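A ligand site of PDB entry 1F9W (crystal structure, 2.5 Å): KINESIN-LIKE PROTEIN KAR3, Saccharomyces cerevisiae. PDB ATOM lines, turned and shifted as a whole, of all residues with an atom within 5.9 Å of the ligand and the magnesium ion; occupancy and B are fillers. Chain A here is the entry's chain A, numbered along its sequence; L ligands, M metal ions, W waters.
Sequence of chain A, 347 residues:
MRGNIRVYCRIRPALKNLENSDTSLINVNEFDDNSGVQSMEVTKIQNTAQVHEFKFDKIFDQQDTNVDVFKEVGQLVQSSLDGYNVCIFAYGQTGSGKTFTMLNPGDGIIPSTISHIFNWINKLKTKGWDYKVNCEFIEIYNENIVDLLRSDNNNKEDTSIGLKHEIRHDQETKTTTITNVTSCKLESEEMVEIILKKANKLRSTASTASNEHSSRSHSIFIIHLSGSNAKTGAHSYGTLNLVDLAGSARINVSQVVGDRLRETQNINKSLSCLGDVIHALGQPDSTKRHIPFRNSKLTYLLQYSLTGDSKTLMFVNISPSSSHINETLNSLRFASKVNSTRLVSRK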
ATOM      1  N   ARG A  10     -16.993 -15.873 -18.371  1.00  0.00           N
ATOM      2  CA  ARG A  10     -15.608 -15.537 -18.161  1.00  0.00           C
ATOM      3  C   ARG A  10     -15.036 -14.928 -19.415  1.00  0.00           C
ATOM      4  O   ARG A  10     -14.664 -15.647 -20.346  1.00  0.00           O
ATOM      5  CB  ARG A  10     -14.823 -16.776 -17.762  1.00  0.00           C
ATOM      6  CG  ARG A  10     -13.329 -16.694 -18.048  1.00  0.00           C
ATOM      7  CD  ARG A  10     -12.538 -16.678 -16.765  1.00  0.00           C
ATOM      8  NE  ARG A  10     -11.482 -15.678 -16.823  1.00  0.00           N
ATOM      9  CZ  ARG A  10     -10.205 -15.908 -16.502  1.00  0.00           C
ATOM     10  NH1 ARG A  10      -9.803 -17.106 -16.097  1.00  0.00           N
ATOM     11  NH2 ARG A  10      -9.325 -14.914 -16.593  1.00  0.00           N
ATOM     12  N   ILE A  11     -15.014 -13.599 -19.448  1.00  0.00           N
ATOM     13  CA  ILE A  11     -14.484 -12.876 -20.569  1.00  0.00           C
ATOM     14  C   ILE A  11     -12.975 -12.889 -20.370  1.00  0.00           C
ATOM     15  O   ILE A  11     -12.476 -13.077 -19.262  1.00  0.00           O
ATOM     16  CB  ILE A  11     -15.016 -11.426 -20.602  1.00  0.00           C
ATOM     17  CG1 ILE A  11     -16.542 -11.423 -20.500  1.00  0.00           C
ATOM     18  CG2 ILE A  11     -14.636 -10.753 -21.898  1.00  0.00           C
ATOM     19  CD1 ILE A  11     -17.039 -11.363 -19.092  1.00  0.00           C
ATOM     20  N   ARG A  12     -12.239 -12.715 -21.455  1.00  0.00           N
ATOM     21  CA  ARG A  12     -10.793 -12.693 -21.395  1.00  0.00           C
ATOM     22  C   ARG A  12     -10.438 -11.438 -22.164  1.00  0.00           C
ATOM     23  O   ARG A  12     -11.282 -10.920 -22.899  1.00  0.00           O
ATOM     24  CB  ARG A  12     -10.206 -13.919 -22.094  1.00  0.00           C
ATOM     25  CG  ARG A  12      -9.996 -13.744 -23.596  1.00  0.00           C
ATOM     26  CD  ARG A  12     -11.318 -13.841 -24.298  1.00  0.00           C
ATOM     27  NE  ARG A  12     -11.281 -13.969 -25.768  1.00  0.00           N
ATOM     28  CZ  ARG A  12     -10.200 -14.156 -26.535  1.00  0.00           C
ATOM     29  NH1 ARG A  12      -8.993 -14.251 -26.007  1.00  0.00           N
ATOM     30  NH2 ARG A  12     -10.361 -14.265 -27.848  1.00  0.00           N
ATOM     31  N   PRO A  13      -9.206 -10.933 -22.010  1.00  0.00           N
ATOM     32  CA  PRO A  13      -8.766  -9.719 -22.712  1.00  0.00           C
ATOM     33  C   PRO A  13      -8.493  -9.984 -24.193  1.00  0.00           C
ATOM     34  O   PRO A  13      -8.040 -11.067 -24.552  1.00  0.00           O
ATOM     35  CB  PRO A  13      -7.490  -9.353 -21.972  1.00  0.00           C
ATOM     36  CG  PRO A  13      -6.952 -10.671 -21.508  1.00  0.00           C
ATOM     37  CD  PRO A  13      -8.159 -11.478 -21.132  1.00  0.00           C
ATOM     38  N   LEU A  15      -6.784  -9.798 -28.051  1.00  0.00           N
ATOM     39  CA  LEU A  15      -5.453 -10.245 -28.481  1.00  0.00           C
ATOM     40  C   LEU A  15      -4.937  -9.538 -29.751  1.00  0.00           C
ATOM     41  O   LEU A  15      -5.614  -8.674 -30.332  1.00  0.00           O
ATOM     42  CB  LEU A  15      -5.466 -11.760 -28.706  1.00  0.00           C
ATOM     43  CG  LEU A  15      -6.175 -12.640 -27.670  1.00  0.00           C
ATOM     44  CD1 LEU A  15      -6.513 -13.993 -28.256  1.00  0.00           C
ATOM     45  CD2 LEU A  15      -5.291 -12.813 -26.450  1.00  0.00           C
ATOM     46  N   GLN A  62     -12.402  -9.595 -18.461  1.00  0.00           N
ATOM     47  CA  GLN A  62     -10.966  -9.765 -18.674  1.00  0.00           C
ATOM     48  C   GLN A  62     -10.082  -9.283 -17.539  1.00  0.00           C
ATOM     49  O   GLN A  62      -8.958  -9.775 -17.374  1.00  0.00           O
ATOM     50  CB  GLN A  62     -10.537  -9.082 -19.970  1.00  0.00           C
ATOM     51  CG  GLN A  62     -10.778  -7.581 -20.023  1.00  0.00           C
ATOM     52  CD  GLN A  62     -11.518  -7.151 -21.281  1.00  0.00           C
ATOM     53  OE1 GLN A  62     -10.923  -7.003 -22.357  1.00  0.00           O
ATOM     54  NE2 GLN A  62     -12.817  -6.965 -21.159  1.00  0.00           N
ATOM     55  N   ASP A  64     -10.537  -9.698 -14.233  1.00  0.00           N
ATOM     56  CA  ASP A  64     -10.354 -10.772 -13.256  1.00  0.00           C
ATOM     57  C   ASP A  64      -9.351 -11.812 -13.742  1.00  0.00           C
ATOM     58  O   ASP A  64      -9.340 -12.187 -14.911  1.00  0.00           O
ATOM     59  CB  ASP A  64     -11.690 -11.438 -12.937  1.00  0.00           C
ATOM     60  CG  ASP A  64     -12.692 -10.466 -12.325  1.00  0.00           C
ATOM     61  OD1 ASP A  64     -12.335  -9.803 -11.328  1.00  0.00           O
ATOM     62  OD2 ASP A  64     -13.842 -10.364 -12.833  1.00  0.00           O
ATOM     63  N   ASN A  66      -6.947 -15.605 -12.968  1.00  0.00           N
ATOM     64  CA  ASN A  66      -7.191 -16.989 -12.602  1.00  0.00           C
ATOM     65  C   ASN A  66      -7.390 -17.085 -11.106  1.00  0.00           C
ATOM     66  O   ASN A  66      -8.278 -17.815 -10.632  1.00  0.00           O
ATOM     67  CB  ASN A  66      -6.021 -17.874 -13.028  1.00  0.00           C
ATOM     68  CG  ASN A  66      -6.143 -18.350 -14.452  1.00  0.00           C
ATOM     69  OD1 ASN A  66      -6.949 -17.829 -15.231  1.00  0.00           O
ATOM     70  ND2 ASN A  66      -5.336 -19.350 -14.817  1.00  0.00           N
ATOM     71  N   GLY A  92     -17.249 -23.096 -24.294  1.00  0.00           N
ATOM     72  CA  GLY A  92     -17.166 -21.876 -25.085  1.00  0.00           C
ATOM     73  C   GLY A  92     -16.339 -22.028 -26.349  1.00  0.00           C
ATOM     74  O   GLY A  92     -15.472 -22.894 -26.419  1.00  0.00           O
ATOM     75  N   GLN A  93     -16.610 -21.169 -27.345  1.00  0.00           N
ATOM     76  CA  GLN A  93     -15.891 -21.181 -28.620  1.00  0.00           C
ATOM     77  C   GLN A  93     -14.357 -21.202 -28.433  1.00  0.00           C
ATOM     78  O   GLN A  93     -13.840 -20.715 -27.437  1.00  0.00           O
ATOM     79  CB  GLN A  93     -16.307 -19.965 -29.455  1.00  0.00           C
ATOM     80  CG  GLN A  93     -15.174 -19.194 -30.099  1.00  0.00           C
ATOM     81  CD  GLN A  93     -15.599 -17.811 -30.562  1.00  0.00           C
ATOM     82  OE1 GLN A  93     -15.740 -17.557 -31.755  1.00  0.00           O
ATOM     83  NE2 GLN A  93     -15.790 -16.905 -29.614  1.00  0.00           N
ATOM     84  N   THR A  94     -13.626 -21.736 -29.408  1.00  0.00           N
ATOM     85  CA  THR A  94     -12.163 -21.859 -29.284  1.00  0.00           C
ATOM     86  C   THR A  94     -11.406 -20.549 -29.211  1.00  0.00           C
ATOM     87  O   THR A  94     -11.785 -19.547 -29.809  1.00  0.00           O
ATOM     88  CB  THR A  94     -11.562 -22.718 -30.419  1.00  0.00           C
ATOM     89  OG1 THR A  94     -12.038 -24.073 -30.315  1.00  0.00           O
ATOM     90  CG2 THR A  94     -10.030 -22.710 -30.336  1.00  0.00           C
ATOM     91  N   GLY A  95     -10.308 -20.572 -28.466  1.00  0.00           N
ATOM     92  CA  GLY A  95      -9.511 -19.369 -28.304  1.00  0.00           C
ATOM     93  C   GLY A  95     -10.129 -18.468 -27.261  1.00  0.00           C
ATOM     94  O   GLY A  95      -9.572 -17.427 -26.933  1.00  0.00           O
ATOM     95  N   SER A  96     -11.285 -18.853 -26.738  1.00  0.00           N
ATOM     96  CA  SER A  96     -11.964 -18.070 -25.723  1.00  0.00           C
ATOM     97  C   SER A  96     -11.371 -18.267 -24.296  1.00  0.00           C
ATOM     98  O   SER A  96     -11.852 -17.650 -23.333  1.00  0.00           O
ATOM     99  CB  SER A  96     -13.462 -18.376 -25.747  1.00  0.00           C
ATOM    100  OG  SER A  96     -13.793 -19.523 -25.003  1.00  0.00           O
ATOM    101  N   GLY A  97     -10.355 -19.127 -24.163  1.00  0.00           N
ATOM    102  CA  GLY A  97      -9.722 -19.326 -22.874  1.00  0.00           C
ATOM    103  C   GLY A  97      -9.840 -20.569 -22.016  1.00  0.00           C
ATOM    104  O   GLY A  97      -9.162 -20.671 -20.980  1.00  0.00           O
ATOM    105  N   LYS A  98     -10.653 -21.525 -22.419  1.00  0.00           N
ATOM    106  CA  LYS A  98     -10.883 -22.754 -21.644  1.00  0.00           C
ATOM    107  C   LYS A  98      -9.643 -23.440 -21.078  1.00  0.00           C
ATOM    108  O   LYS A  98      -9.595 -23.812 -19.906  1.00  0.00           O
ATOM    109  CB  LYS A  98     -11.673 -23.750 -22.504  1.00  0.00           C
ATOM    110  CG  LYS A  98     -12.659 -23.051 -23.430  1.00  0.00           C
ATOM    111  CD  LYS A  98     -13.655 -24.025 -24.027  1.00  0.00           C
ATOM    112  CE  LYS A  98     -13.030 -24.752 -25.205  1.00  0.00           C
ATOM    113  NZ  LYS A  98     -12.698 -23.812 -26.312  1.00  0.00           N
ATOM    114  N   THR A  99      -8.644 -23.616 -21.909  1.00  0.00           N
ATOM    115  CA  THR A  99      -7.452 -24.271 -21.450  1.00  0.00           C
ATOM    116  C   THR A  99      -6.676 -23.383 -20.492  1.00  0.00           C
ATOM    117  O   THR A  99      -5.987 -23.897 -19.595  1.00  0.00           O
ATOM    118  CB  THR A  99      -6.557 -24.612 -22.630  1.00  0.00           C
ATOM    119  OG1 THR A  99      -7.354 -25.096 -23.720  1.00  0.00           O
ATOM    120  CG2 THR A  99      -5.554 -25.664 -22.207  1.00  0.00           C
ATOM    121  N   PHE A 100      -6.782 -22.067 -20.675  1.00  0.00           N
ATOM    122  CA  PHE A 100      -6.072 -21.098 -19.820  1.00  0.00           C
ATOM    123  C   PHE A 100      -6.665 -21.146 -18.425  1.00  0.00           C
ATOM    124  O   PHE A 100      -5.947 -21.311 -17.433  1.00  0.00           O
ATOM    125  CB  PHE A 100      -6.236 -19.689 -20.405  1.00  0.00           C
ATOM    126  CG  PHE A 100      -5.491 -18.612 -19.627  1.00  0.00           C
ATOM    127  CD1 PHE A 100      -6.037 -18.066 -18.450  1.00  0.00           C
ATOM    128  CD2 PHE A 100      -4.266 -18.120 -20.069  1.00  0.00           C
ATOM    129  CE1 PHE A 100      -5.365 -17.066 -17.755  1.00  0.00           C
ATOM    130  CE2 PHE A 100      -3.593 -17.119 -19.374  1.00  0.00           C
ATOM    131  CZ  PHE A 100      -4.150 -16.600 -18.228  1.00  0.00           C
ATOM    132  N   THR A 101      -7.983 -20.999 -18.369  1.00  0.00           N
ATOM    133  CA  THR A 101      -8.736 -21.027 -17.143  1.00  0.00           C
ATOM    134  C   THR A 101      -8.436 -22.288 -16.358  1.00  0.00           C
ATOM    135  O   THR A 101      -8.363 -22.274 -15.124  1.00  0.00           O
ATOM    136  CB  THR A 101     -10.241 -21.043 -17.467  1.00  0.00           C
ATOM    137  OG1 THR A 101     -10.560 -19.962 -18.348  1.00  0.00           O
ATOM    138  CG2 THR A 101     -11.076 -20.931 -16.195  1.00  0.00           C
ATOM    139  N   ASN A 104      -3.671 -22.904 -17.220  1.00  0.00           N
ATOM    140  CA  ASN A 104      -2.656 -21.859 -17.247  1.00  0.00           C
ATOM    141  C   ASN A 104      -1.720 -22.207 -16.094  1.00  0.00           C
ATOM    142  O   ASN A 104      -2.177 -22.413 -14.974  1.00  0.00           O
ATOM    143  CB  ASN A 104      -3.274 -20.472 -17.018  1.00  0.00           C
ATOM    144  CG  ASN A 104      -2.276 -19.353 -17.267  1.00  0.00           C
ATOM    145  OD1 ASN A 104      -1.728 -19.239 -18.373  1.00  0.00           O
ATOM    146  ND2 ASN A 104      -2.030 -18.529 -16.251  1.00  0.00           N
ATOM    147  N   ARG A 203      -2.750 -29.295 -24.194  1.00  0.00           N
ATOM    148  CA  ARG A 203      -3.921 -28.469 -24.501  1.00  0.00           C
ATOM    149  C   ARG A 203      -3.682 -26.998 -24.915  1.00  0.00           C
ATOM    150  O   ARG A 203      -4.594 -26.164 -24.796  1.00  0.00           O
ATOM    151  CB  ARG A 203      -4.886 -28.509 -23.306  1.00  0.00           C
ATOM    152  CG  ARG A 203      -4.908 -29.828 -22.564  1.00  0.00           C
ATOM    153  CD  ARG A 203      -5.894 -30.783 -23.201  1.00  0.00           C
ATOM    154  NE  ARG A 203      -7.121 -30.101 -23.606  1.00  0.00           N
ATOM    155  CZ  ARG A 203      -8.058 -30.632 -24.387  1.00  0.00           C
ATOM    156  NH1 ARG A 203      -7.902 -31.878 -24.836  1.00  0.00           N
ATOM    157  NH2 ARG A 203      -9.148 -29.930 -24.703  1.00  0.00           N
ATOM    158  N   SER A 204      -2.485 -26.674 -25.403  1.00  0.00           N
ATOM    159  CA  SER A 204      -2.170 -25.311 -25.825  1.00  0.00           C
ATOM    160  C   SER A 204      -1.668 -25.232 -27.267  1.00  0.00           C
ATOM    161  O   SER A 204      -1.671 -26.232 -27.969  1.00  0.00           O
ATOM    162  CB  SER A 204      -1.121 -24.723 -24.884  1.00  0.00           C
ATOM    163  OG  SER A 204      -1.720 -23.955 -23.858  1.00  0.00           O
ATOM    164  N   SER A 214      -6.761 -30.383 -29.427  1.00  0.00           N
ATOM    165  CA  SER A 214      -7.238 -30.110 -28.078  1.00  0.00           C
ATOM    166  C   SER A 214      -8.523 -29.296 -28.219  1.00  0.00           C
ATOM    167  O   SER A 214      -9.350 -29.199 -27.303  1.00  0.00           O
ATOM    168  CB  SER A 214      -6.181 -29.302 -27.301  1.00  0.00           C
ATOM    169  OG  SER A 214      -5.284 -28.603 -28.169  1.00  0.00           O
ATOM    170  N   SER A 215      -8.676 -28.711 -29.397  1.00  0.00           N
ATOM    171  CA  SER A 215      -9.825 -27.889 -29.699  1.00  0.00           C
ATOM    172  C   SER A 215     -11.061 -28.713 -29.994  1.00  0.00           C
ATOM    173  O   SER A 215     -12.179 -28.321 -29.636  1.00  0.00           O
ATOM    174  CB  SER A 215      -9.519 -27.003 -30.905  1.00  0.00           C
ATOM    175  OG  SER A 215     -10.708 -26.412 -31.389  1.00  0.00           O
ATOM    176  N   ASP A 244     -12.225 -29.640 -19.723  1.00  0.00           N
ATOM    177  CA  ASP A 244     -11.920 -28.660 -20.742  1.00  0.00           C
ATOM    178  C   ASP A 244     -12.719 -29.181 -21.938  1.00  0.00           C
ATOM    179  O   ASP A 244     -12.266 -30.086 -22.656  1.00  0.00           O
ATOM    180  CB  ASP A 244     -10.414 -28.697 -21.020  1.00  0.00           C
ATOM    181  CG  ASP A 244      -9.951 -27.609 -21.963  1.00  0.00           C
ATOM    182  OD1 ASP A 244     -10.785 -26.823 -22.482  1.00  0.00           O
ATOM    183  OD2 ASP A 244      -8.725 -27.521 -22.192  1.00  0.00           O
ATOM    184  N   ASN A 317     -16.495 -19.559 -21.151  1.00  0.00           N
ATOM    185  CA  ASN A 317     -15.427 -18.671 -21.564  1.00  0.00           C
ATOM    186  C   ASN A 317     -15.842 -17.983 -22.842  1.00  0.00           C
ATOM    187  O   ASN A 317     -16.146 -18.627 -23.835  1.00  0.00           O
ATOM    188  CB  ASN A 317     -14.135 -19.448 -21.818  1.00  0.00           C
ATOM    189  CG  ASN A 317     -13.682 -20.248 -20.608  1.00  0.00           C
ATOM    190  OD1 ASN A 317     -14.479 -20.591 -19.743  1.00  0.00           O
ATOM    191  ND2 ASN A 317     -12.399 -20.530 -20.545  1.00  0.00           N
HETATM  192  P1  LIG L   1      -9.446 -21.990 -25.707  1.00  0.00           P
HETATM  193  O1  LIG L   1     -10.824 -21.452 -25.581  1.00  0.00           O
HETATM  194  O2  LIG L   1      -9.189 -23.149 -24.605  1.00  0.00           O
HETATM  195  O3  LIG L   1      -9.157 -22.463 -27.108  1.00  0.00           O
HETATM  196  P2  LIG L   1      -6.957 -21.064 -24.717  1.00  0.00           P
HETATM  197  O4  LIG L   1      -7.093 -20.902 -23.266  1.00  0.00           O
HETATM  198  O5  LIG L   1      -6.407 -22.376 -25.079  1.00  0.00           O
HETATM  199  O6  LIG L   1      -8.384 -20.919 -25.342  1.00  0.00           O
HETATM  200  O7  LIG L   1      -6.096 -19.906 -25.354  1.00  0.00           O
HETATM  201  C1  LIG L   1      -6.605 -18.921 -26.259  1.00  0.00           C
HETATM  202  C2  LIG L   1      -5.723 -17.656 -26.130  1.00  0.00           C
HETATM  203  O8  LIG L   1      -6.406 -16.726 -25.256  1.00  0.00           O
HETATM  204  C3  LIG L   1      -4.347 -17.912 -25.491  1.00  0.00           C
HETATM  205  O9  LIG L   1      -3.294 -17.187 -26.154  1.00  0.00           O
HETATM  206  C4  LIG L   1      -4.510 -17.464 -24.045  1.00  0.00           C
HETATM  207  O10 LIG L   1      -3.270 -17.099 -23.414  1.00  0.00           O
HETATM  208  C5  LIG L   1      -5.566 -16.370 -24.131  1.00  0.00           C
HETATM  209  N1  LIG L   1      -6.380 -16.274 -22.875  1.00  0.00           N
HETATM  210  C6  LIG L   1      -7.456 -17.011 -22.587  1.00  0.00           C
HETATM  211  N2  LIG L   1      -7.926 -16.685 -21.389  1.00  0.00           N
HETATM  212  C7  LIG L   1      -7.156 -15.750 -20.891  1.00  0.00           C
HETATM  213  C8  LIG L   1      -7.104 -15.028 -19.699  1.00  0.00           C
HETATM  214  N3  LIG L   1      -8.026 -15.224 -18.759  1.00  0.00           N
HETATM  215  N4  LIG L   1      -6.136 -14.085 -19.502  1.00  0.00           N
HETATM  216  C9  LIG L   1      -5.180 -13.842 -20.425  1.00  0.00           C
HETATM  217  N5  LIG L   1      -5.211 -14.545 -21.582  1.00  0.00           N
HETATM  218  C10 LIG L   1      -6.152 -15.487 -21.847  1.00  0.00           C
HETATM  219 MG    MG M   1      -8.065 -25.045 -26.051  1.00  0.00          MG
HETATM  220  O   HOH W   1     -10.057 -17.268 -19.791  1.00  0.00           O
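O2 of the ligand is in hydrogen-bond range of N of Lys 98.
An oxygen (O4) of the ligand sits close to the backbone carbonyl oxygen (O) of Gly 97.
N3 of the ligand sits close to NH2 of Arg 10, at 2.5 Å.
N of Phe 100 lies within hydrogen-bond range of O4 of the ligand, 2.9 Å away.
O2 of the ligand lies close to OG1 of Thr 99 (2.8 Å).
N of Thr 99 sits at hydrogen-bond distance from O2 of the ligand, at 2.8 Å.
O1 of the ligand sits at hydrogen-bond distance from N of Ser 96.
An oxygen (O1) of the ligand lies within hydrogen-bond range of the backbone NH of Gly 97.
An oxygen (O3) of the ligand is in hydrogen-bond range of the backbone NH of Gly 95 (2.6 Å).
The side-chain amino group (NZ) of Lys 98 is in salt-bridge range of an oxygen (O1) of the ligand (3.1 Å).
The guanidinium group (NH1) of Arg 10 lies within hydrogen-bond range of the side-chain amide oxygen (OD1) of Asn 66, at 3.1 Å.
O of Asn 317 is in hydrogen-bond range of OG of Ser 96 (2.8 Å).
The backbone carbonyl oxygen (O) of Gln 93 lies within hydrogen-bond range of the side-chain amino group (NZ) of Lys 98 (3.5 Å).
O of Thr 99 is in hydrogen-bond range of N of Asn 104.
The backbone carbonyl oxygen (O) of Ser 214 sits at hydrogen-bond distance from the guanidinium group (NH2) of Arg 203 (2.7 Å).
The side-chain hydroxyl of Ser 96 lies within hydrogen-bond range of the backbone carbonyl oxygen of Gln 93.
The backbone carbonyl oxygen of Gly 97 lies close to the side-chain amide nitrogen of Asn 317 (3.3 Å).
The side-chain hydroxyl (OG1) of Thr 99 lies close to the backbone carbonyl oxygen (O) of Arg 203 (3.1 Å).
Residues that only touch the ligand: Thr 94 (3.4 Å), Gln 93 (3.6 Å), Arg 12 (3.7 Å) and Pro 13 (3.7 Å).
Hydrophobic or aromatic side chains that line the ligand: Pro 13 and Phe 100.
11 residues have an atom within 4 Å of the ligand: Arg 10, Arg 12, Pro 13, Gln 93, Thr 94, Gly 95, Ser 96, Gly 97, Lys 98, Thr 99 and Phe 100.
The nearest printed residue that does not touch the ligand is Leu 15 (4.1 Å).
Merely in contact with the magnesium ion: Arg 203.
Of the 25 residues printed, 2 come within 4 Å of the magnesium ion.
The magnesium ion is bound by OG1 of Thr 99 (2.4 Å).
Slightly farther from the magnesium ion lies an oxygen (O2) of the ligand (2.6 Å).
Water W1 bridges N2 of the ligand (2.7 Å) and OG1 of Thr 101 (3.1 Å).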
